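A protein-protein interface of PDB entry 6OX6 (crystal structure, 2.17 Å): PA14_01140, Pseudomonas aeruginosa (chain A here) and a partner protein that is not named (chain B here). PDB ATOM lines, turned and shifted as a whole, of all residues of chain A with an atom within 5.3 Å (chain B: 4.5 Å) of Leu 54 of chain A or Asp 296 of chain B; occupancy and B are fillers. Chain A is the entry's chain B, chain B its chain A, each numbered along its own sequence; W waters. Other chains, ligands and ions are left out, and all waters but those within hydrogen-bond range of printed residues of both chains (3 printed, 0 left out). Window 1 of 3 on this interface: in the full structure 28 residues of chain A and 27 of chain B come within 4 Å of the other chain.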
ATOM      1  N   TYR A  18      13.901 -14.530 -10.398  1.00  0.00           N
ATOM      2  CA  TYR A  18      14.812 -15.379  -9.625  1.00  0.00           C
ATOM      3  C   TYR A  18      15.225 -14.549  -8.418  1.00  0.00           C
ATOM      4  O   TYR A  18      16.183 -13.770  -8.503  1.00  0.00           O
ATOM      5  CB  TYR A  18      16.014 -15.793 -10.481  1.00  0.00           C
ATOM      6  CG  TYR A  18      17.061 -16.683  -9.803  1.00  0.00           C
ATOM      7  CD1 TYR A  18      16.721 -17.564  -8.763  1.00  0.00           C
ATOM      8  CD2 TYR A  18      18.398 -16.649 -10.223  1.00  0.00           C
ATOM      9  CE1 TYR A  18      17.689 -18.386  -8.154  1.00  0.00           C
ATOM     10  CE2 TYR A  18      19.360 -17.463  -9.613  1.00  0.00           C
ATOM     11  CZ  TYR A  18      18.982 -18.337  -8.598  1.00  0.00           C
ATOM     12  OH  TYR A  18      19.940 -19.120  -8.003  1.00  0.00           O
ATOM     13  N   GLU A  21      19.019 -14.176  -6.677  1.00  0.00           N
ATOM     14  CA  GLU A  21      19.996 -13.223  -7.202  1.00  0.00           C
ATOM     15  C   GLU A  21      19.350 -11.933  -7.694  1.00  0.00           C
ATOM     16  O   GLU A  21      19.939 -11.223  -8.510  1.00  0.00           O
ATOM     17  CB  GLU A  21      20.837 -13.843  -8.327  1.00  0.00           C
ATOM     18  CG  GLU A  21      21.686 -15.072  -7.919  1.00  0.00           C
ATOM     19  CD  GLU A  21      23.118 -15.035  -8.436  1.00  0.00           C
ATOM     20  OE1 GLU A  21      23.651 -13.943  -8.755  1.00  0.00           O
ATOM     21  OE2 GLU A  21      23.705 -16.125  -8.567  1.00  0.00           O
ATOM     22  N   VAL A  23      17.184 -10.982  -9.862  1.00  0.00           N
ATOM     23  CA  VAL A  23      17.281 -10.855 -11.309  1.00  0.00           C
ATOM     24  C   VAL A  23      15.994 -11.372 -11.948  1.00  0.00           C
ATOM     25  O   VAL A  23      15.328 -12.271 -11.410  1.00  0.00           O
ATOM     26  CB  VAL A  23      18.543 -11.579 -11.855  1.00  0.00           C
ATOM     27  CG1 VAL A  23      18.553 -13.121 -11.544  1.00  0.00           C
ATOM     28  CG2 VAL A  23      18.728 -11.292 -13.319  1.00  0.00           C
ATOM     29  N   TYR A  25      14.265 -12.140 -16.142  1.00  0.00           N
ATOM     30  CA  TYR A  25      14.566 -12.389 -17.543  1.00  0.00           C
ATOM     31  C   TYR A  25      13.289 -12.301 -18.356  1.00  0.00           C
ATOM     32  O   TYR A  25      12.183 -12.573 -17.852  1.00  0.00           O
ATOM     33  CB  TYR A  25      15.212 -13.780 -17.776  1.00  0.00           C
ATOM     34  CG  TYR A  25      16.590 -13.906 -17.153  1.00  0.00           C
ATOM     35  CD1 TYR A  25      16.748 -14.437 -15.888  1.00  0.00           C
ATOM     36  CD2 TYR A  25      17.719 -13.446 -17.813  1.00  0.00           C
ATOM     37  CE1 TYR A  25      17.985 -14.540 -15.314  1.00  0.00           C
ATOM     38  CE2 TYR A  25      18.958 -13.552 -17.255  1.00  0.00           C
ATOM     39  CZ  TYR A  25      19.089 -14.095 -16.010  1.00  0.00           C
ATOM     40  OH  TYR A  25      20.326 -14.204 -15.439  1.00  0.00           O
ATOM     41  N   PHE A  38      17.816  -6.622 -13.906  1.00  0.00           N
ATOM     42  CA  PHE A  38      18.129  -6.777 -12.489  1.00  0.00           C
ATOM     43  C   PHE A  38      17.216  -5.907 -11.655  1.00  0.00           C
ATOM     44  O   PHE A  38      16.726  -4.877 -12.124  1.00  0.00           O
ATOM     45  CB  PHE A  38      19.583  -6.417 -12.205  1.00  0.00           C
ATOM     46  CG  PHE A  38      20.573  -7.419 -12.781  1.00  0.00           C
ATOM     47  CD1 PHE A  38      21.162  -7.205 -14.019  1.00  0.00           C
ATOM     48  CD2 PHE A  38      20.885  -8.567 -12.092  1.00  0.00           C
ATOM     49  CE1 PHE A  38      22.042  -8.110 -14.553  1.00  0.00           C
ATOM     50  CE2 PHE A  38      21.788  -9.508 -12.636  1.00  0.00           C
ATOM     51  CZ  PHE A  38      22.352  -9.266 -13.861  1.00  0.00           C
ATOM     52  N   ASN A  52      24.044 -19.251 -20.646  1.00  0.00           N
ATOM     53  CA  ASN A  52      24.565 -18.407 -19.573  1.00  0.00           C
ATOM     54  C   ASN A  52      24.280 -19.022 -18.202  1.00  0.00           C
ATOM     55  O   ASN A  52      23.187 -19.521 -17.940  1.00  0.00           O
ATOM     56  CB  ASN A  52      23.934 -17.022 -19.657  1.00  0.00           C
ATOM     57  CG  ASN A  52      24.299 -16.149 -18.494  1.00  0.00           C
ATOM     58  OD1 ASN A  52      23.538 -16.013 -17.517  1.00  0.00           O
ATOM     59  ND2 ASN A  52      25.473 -15.554 -18.575  1.00  0.00           N
ATOM     60  N   ARG A  53      25.270 -18.958 -17.313  1.00  0.00           N
ATOM     61  CA  ARG A  53      25.174 -19.602 -16.005  1.00  0.00           C
ATOM     62  C   ARG A  53      23.969 -19.093 -15.214  1.00  0.00           C
ATOM     63  O   ARG A  53      23.161 -19.876 -14.707  1.00  0.00           O
ATOM     64  CB  ARG A  53      26.472 -19.345 -15.229  1.00  0.00           C
ATOM     65  CG  ARG A  53      26.667 -20.226 -13.995  1.00  0.00           C
ATOM     66  CD  ARG A  53      25.997 -19.641 -12.734  1.00  0.00           C
ATOM     67  NE  ARG A  53      26.279 -18.214 -12.529  1.00  0.00           N
ATOM     68  CZ  ARG A  53      25.773 -17.485 -11.530  1.00  0.00           C
ATOM     69  NH1 ARG A  53      24.941 -18.041 -10.660  1.00  0.00           N
ATOM     70  NH2 ARG A  53      26.075 -16.192 -11.408  1.00  0.00           N
ATOM     71  N   LEU A  54      23.871 -17.781 -15.049  1.00  0.00           N
ATOM     72  CA  LEU A  54      22.848 -17.229 -14.162  1.00  0.00           C
ATOM     73  C   LEU A  54      21.457 -17.439 -14.752  1.00  0.00           C
ATOM     74  O   LEU A  54      20.498 -17.759 -14.035  1.00  0.00           O
ATOM     75  CB  LEU A  54      23.147 -15.746 -13.921  1.00  0.00           C
ATOM     76  CG  LEU A  54      22.202 -14.909 -13.050  1.00  0.00           C
ATOM     77  CD1 LEU A  54      22.164 -15.501 -11.645  1.00  0.00           C
ATOM     78  CD2 LEU A  54      22.643 -13.414 -13.036  1.00  0.00           C
ATOM     79  N   PHE A  55      21.343 -17.354 -16.075  1.00  0.00           N
ATOM     80  CA  PHE A  55      20.071 -17.660 -16.719  1.00  0.00           C
ATOM     81  C   PHE A  55      19.620 -19.096 -16.446  1.00  0.00           C
ATOM     82  O   PHE A  55      18.455 -19.339 -16.108  1.00  0.00           O
ATOM     83  CB  PHE A  55      20.177 -17.438 -18.222  1.00  0.00           C
ATOM     84  CG  PHE A  55      18.931 -17.873 -18.969  1.00  0.00           C
ATOM     85  CD1 PHE A  55      17.735 -17.186 -18.790  1.00  0.00           C
ATOM     86  CD2 PHE A  55      18.945 -18.985 -19.810  1.00  0.00           C
ATOM     87  CE1 PHE A  55      16.589 -17.566 -19.457  1.00  0.00           C
ATOM     88  CE2 PHE A  55      17.781 -19.378 -20.484  1.00  0.00           C
ATOM     89  CZ  PHE A  55      16.609 -18.669 -20.307  1.00  0.00           C
ATOM     90  N   ASN A  56      20.519 -20.065 -16.633  1.00  0.00           N
ATOM     91  CA  ASN A  56      20.152 -21.445 -16.349  1.00  0.00           C
ATOM     92  C   ASN A  56      19.878 -21.660 -14.859  1.00  0.00           C
ATOM     93  O   ASN A  56      19.050 -22.499 -14.500  1.00  0.00           O
ATOM     94  CB  ASN A  56      21.246 -22.386 -16.861  1.00  0.00           C
ATOM     95  CG  ASN A  56      21.159 -22.580 -18.379  1.00  0.00           C
ATOM     96  OD1 ASN A  56      20.446 -23.462 -18.845  1.00  0.00           O
ATOM     97  ND2 ASN A  56      21.852 -21.749 -19.142  1.00  0.00           N
ATOM     98  N   ASP A  57      20.530 -20.896 -13.973  1.00  0.00           N
ATOM     99  CA  ASP A  57      20.131 -20.953 -12.563  1.00  0.00           C
ATOM    100  C   ASP A  57      18.704 -20.452 -12.388  1.00  0.00           C
ATOM    101  O   ASP A  57      17.925 -21.016 -11.603  1.00  0.00           O
ATOM    102  CB  ASP A  57      21.092 -20.150 -11.683  1.00  0.00           C
ATOM    103  CG  ASP A  57      22.358 -20.928 -11.327  1.00  0.00           C
ATOM    104  OD1 ASP A  57      22.503 -22.068 -11.790  1.00  0.00           O
ATOM    105  OD2 ASP A  57      23.212 -20.409 -10.568  1.00  0.00           O
ATOM    106  N   ALA A  58      18.354 -19.383 -13.100  1.00  0.00           N
ATOM    107  CA  ALA A  58      17.009 -18.823 -13.023  1.00  0.00           C
ATOM    108  C   ALA A  58      15.977 -19.824 -13.499  1.00  0.00           C
ATOM    109  O   ALA A  58      14.893 -19.932 -12.914  1.00  0.00           O
ATOM    110  CB  ALA A  58      16.934 -17.536 -13.841  1.00  0.00           C
ATOM    111  N   LEU A  59      16.308 -20.608 -14.527  1.00  0.00           N
ATOM    112  CA  LEU A  59      15.371 -21.640 -14.969  1.00  0.00           C
ATOM    113  C   LEU A  59      15.187 -22.694 -13.904  1.00  0.00           C
ATOM    114  O   LEU A  59      14.069 -23.185 -13.699  1.00  0.00           O
ATOM    115  CB  LEU A  59      15.842 -22.306 -16.253  1.00  0.00           C
ATOM    116  CG  LEU A  59      16.027 -21.367 -17.431  1.00  0.00           C
ATOM    117  CD1 LEU A  59      16.313 -22.164 -18.714  1.00  0.00           C
ATOM    118  CD2 LEU A  59      14.790 -20.521 -17.599  1.00  0.00           C
ATOM    119  N   LYS B 292      32.848 -13.628 -15.447  1.00  0.00           N
ATOM    120  CA  LYS B 292      31.551 -13.870 -14.808  1.00  0.00           C
ATOM    121  C   LYS B 292      30.811 -12.561 -14.533  1.00  0.00           C
ATOM    122  O   LYS B 292      29.590 -12.469 -14.738  1.00  0.00           O
ATOM    123  CB  LYS B 292      31.751 -14.665 -13.520  1.00  0.00           C
ATOM    124  CG  LYS B 292      30.470 -15.025 -12.803  1.00  0.00           C
ATOM    125  CD  LYS B 292      30.744 -16.039 -11.709  1.00  0.00           C
ATOM    126  CE  LYS B 292      29.457 -16.657 -11.177  1.00  0.00           C
ATOM    127  NZ  LYS B 292      29.770 -17.733 -10.196  1.00  0.00           N
ATOM    128  N   ILE B 293      31.528 -11.530 -14.081  1.00  0.00           N
ATOM    129  CA  ILE B 293      30.903 -10.215 -13.910  1.00  0.00           C
ATOM    130  C   ILE B 293      30.360  -9.700 -15.232  1.00  0.00           C
ATOM    131  O   ILE B 293      29.245  -9.165 -15.296  1.00  0.00           O
ATOM    132  CB  ILE B 293      31.908  -9.215 -13.316  1.00  0.00           C
ATOM    133  CG1 ILE B 293      32.117  -9.534 -11.836  1.00  0.00           C
ATOM    134  CG2 ILE B 293      31.419  -7.759 -13.565  1.00  0.00           C
ATOM    135  CD1 ILE B 293      33.441  -8.951 -11.262  1.00  0.00           C
ATOM    136  N   ASN B 294      31.160  -9.808 -16.301  1.00  0.00           N
ATOM    137  CA  ASN B 294      30.734  -9.294 -17.598  1.00  0.00           C
ATOM    138  C   ASN B 294      29.576 -10.096 -18.192  1.00  0.00           C
ATOM    139  O   ASN B 294      28.682  -9.511 -18.819  1.00  0.00           O
ATOM    140  CB  ASN B 294      31.914  -9.278 -18.574  1.00  0.00           C
ATOM    141  CG  ASN B 294      32.985  -8.252 -18.188  1.00  0.00           C
ATOM    142  OD1 ASN B 294      32.700  -7.261 -17.522  1.00  0.00           O
ATOM    143  ND2 ASN B 294      34.225  -8.497 -18.622  1.00  0.00           N
ATOM    144  N   ASN B 295      29.578 -11.430 -18.036  1.00  0.00           N
ATOM    145  CA  ASN B 295      28.570 -12.276 -18.671  1.00  0.00           C
ATOM    146  C   ASN B 295      27.302 -12.423 -17.837  1.00  0.00           C
ATOM    147  O   ASN B 295      26.198 -12.193 -18.340  1.00  0.00           O
ATOM    148  CB  ASN B 295      29.129 -13.667 -18.954  1.00  0.00           C
ATOM    149  CG  ASN B 295      30.121 -13.662 -20.084  1.00  0.00           C
ATOM    150  OD1 ASN B 295      29.943 -12.959 -21.086  1.00  0.00           O
ATOM    151  ND2 ASN B 295      31.197 -14.419 -19.919  1.00  0.00           N
ATOM    152  N   ASP B 296      27.435 -12.866 -16.586  1.00  0.00           N
ATOM    153  CA  ASP B 296      26.250 -13.009 -15.751  1.00  0.00           C
ATOM    154  C   ASP B 296      25.674 -11.668 -15.340  1.00  0.00           C
ATOM    155  O   ASP B 296      24.445 -11.505 -15.291  1.00  0.00           O
ATOM    156  CB  ASP B 296      26.565 -13.828 -14.501  1.00  0.00           C
ATOM    157  CG  ASP B 296      26.822 -15.298 -14.816  1.00  0.00           C
ATOM    158  OD1 ASP B 296      26.514 -15.757 -15.958  1.00  0.00           O
ATOM    159  OD2 ASP B 296      27.305 -15.999 -13.894  1.00  0.00           O
ATOM    160  N   TYR B 297      26.539 -10.707 -15.014  1.00  0.00           N
ATOM    161  CA  TYR B 297      26.096  -9.509 -14.326  1.00  0.00           C
ATOM    162  C   TYR B 297      26.253  -8.254 -15.162  1.00  0.00           C
ATOM    163  O   TYR B 297      26.153  -7.148 -14.611  1.00  0.00           O
ATOM    164  CB  TYR B 297      26.840  -9.382 -13.004  1.00  0.00           C
ATOM    165  CG  TYR B 297      26.567 -10.551 -12.111  1.00  0.00           C
ATOM    166  CD1 TYR B 297      25.283 -10.776 -11.596  1.00  0.00           C
ATOM    167  CD2 TYR B 297      27.571 -11.446 -11.795  1.00  0.00           C
ATOM    168  CE1 TYR B 297      25.019 -11.874 -10.768  1.00  0.00           C
ATOM    169  CE2 TYR B 297      27.324 -12.547 -10.981  1.00  0.00           C
ATOM    170  CZ  TYR B 297      26.050 -12.762 -10.468  1.00  0.00           C
ATOM    171  OH  TYR B 297      25.829 -13.868  -9.645  1.00  0.00           O
ATOM    172  N   LYS B 298      26.486  -8.402 -16.466  1.00  0.00           N
ATOM    173  CA  LYS B 298      26.540  -7.287 -17.423  1.00  0.00           C
ATOM    174  C   LYS B 298      27.507  -6.189 -16.987  1.00  0.00           C
ATOM    175  O   LYS B 298      27.248  -5.003 -17.184  1.00  0.00           O
ATOM    176  CB  LYS B 298      25.146  -6.703 -17.680  1.00  0.00           C
ATOM    177  CG  LYS B 298      24.172  -7.704 -18.303  1.00  0.00           C
ATOM    178  CD  LYS B 298      24.735  -8.424 -19.541  1.00  0.00           C
ATOM    179  CE  LYS B 298      23.589  -8.987 -20.402  1.00  0.00           C
ATOM    180  NZ  LYS B 298      24.139  -9.738 -21.607  1.00  0.00           N
HETATM  181  O   HOH W   1      22.460 -13.335 -16.913  1.00  0.00           O
HETATM  182  O   HOH W   2      27.522 -18.722  -8.798  1.00  0.00           O
HETATM  183  O   HOH W   3      27.919 -17.921 -17.916  1.00  0.00           O
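The backbone carbonyl oxygen (O) of Asn 295 of chain B sits at hydrogen-bond distance from the side-chain amide nitrogen (ND2) of Asn 52 of chain A, 3.4 Å away.
The side-chain carboxylate (OD1) of Asp 296 of chain B sits at hydrogen-bond distance from the side-chain amide nitrogen (ND2) of Asn 52 of chain A (2.8 Å).
OD2 of Asp 296 of chain B lies within salt-bridge range of NH2 of Arg 53 of chain A.
OD1 of Asp 296 of chain B is in hydrogen-bond range of N of Leu 54 of chain A, 3.5 Å away.
The side-chain carboxylate (OE2) of Glu 21 of chain A lies close to the side-chain hydroxyl (OH) of Tyr 297 of chain B, 3.3 Å away.
NH2 of Arg 53 of chain A sits at hydrogen-bond distance from OH of Tyr 297 of chain B (2.9 Å).
Of the printed residues of chain B, Glu 21 of chain A touches Tyr 297.
Tyr 25 of chain A touches none of the printed residues of chain B.
Of the printed residues of chain B, Asn 52 of chain A touches Asn 295 (3.4 Å) and Asp 296 (2.8 Å).
Of chain B, only Asp 296 and Tyr 297 come within 4 Å of Leu 54 of chain A.
Printed residues of chain A within 4 Å of Lys 292 of chain B: Arg 53.
Printed residues of chain A within 4 Å of Asn 295 of chain B: Asn 52 (3.4 Å).
Of the printed residues of chain A, Asp 296 of chain B touches Phe 38, Asn 52, Arg 53 and Leu 54.
The nearest printed residue of chain B that does not touch Leu 54 of chain A is Asn 295 of chain B (6.4 Å).
Water W1 lies within hydrogen-bond range of OH of Tyr 25 of chain A (2.7 Å), OD1 of Asn 52 of chain A (2.9 Å) and O of Asp 296 of chain B (3.1 Å).
Water W2 bridges NZ of Lys 292 of chain B and NH1 of Arg 53 of chain A.
Water W3 lies within hydrogen-bond range of N of Arg 53 of chain A, OD1 of Asp 296 of chain B and ND2 of Asn 52 of chain A.
Hydrophobic or aromatic side chains of chain A that line the printed part of chain B: Phe 38 and Leu 54.
Printed residues of chain B that touch a printed residue of chain A: Lys 292, Asn 295, Asp 296 and Tyr 297.
Hydrophobic or aromatic side chains of chain B that line the printed part of chain A: Tyr 297.
Among the printed residues, 10 pairs touch across the chains.
CZ of Phe 38 of chain A touches O of Asp 296 of chain B, at 3.4 Å.
CZ of Phe 38 of chain A touches CA of Tyr 297 of chain B (3.8 Å).
Arg 53 of chain A touches Lys 292 of chain B.
Leu 54 of chain A touches Tyr 297 of chain B.
NH1 of Arg 53 of chain A lies within salt-bridge range of OE2 of Glu 21 of chain A (3.1 Å).
The side-chain amide oxygen of Asn 52 of chain A is in hydrogen-bond range of the backbone NH of Leu 54 of chain A (3.1 Å).
OD1 of Asn 52 of chain A sits at hydrogen-bond distance from N of Phe 55 of chain A (2.9 Å).
The backbone carbonyl oxygen (O) of Asn 52 of chain A sits at hydrogen-bond distance from the side-chain amide nitrogen (ND2) of Asn 56 of chain A, 2.9 Å away.
The guanidinium group (NH1) of Arg 53 of chain A lies within salt-bridge range of the side-chain carboxylate (OD2) of Asp 57 of chain A, at 2.9 Å.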
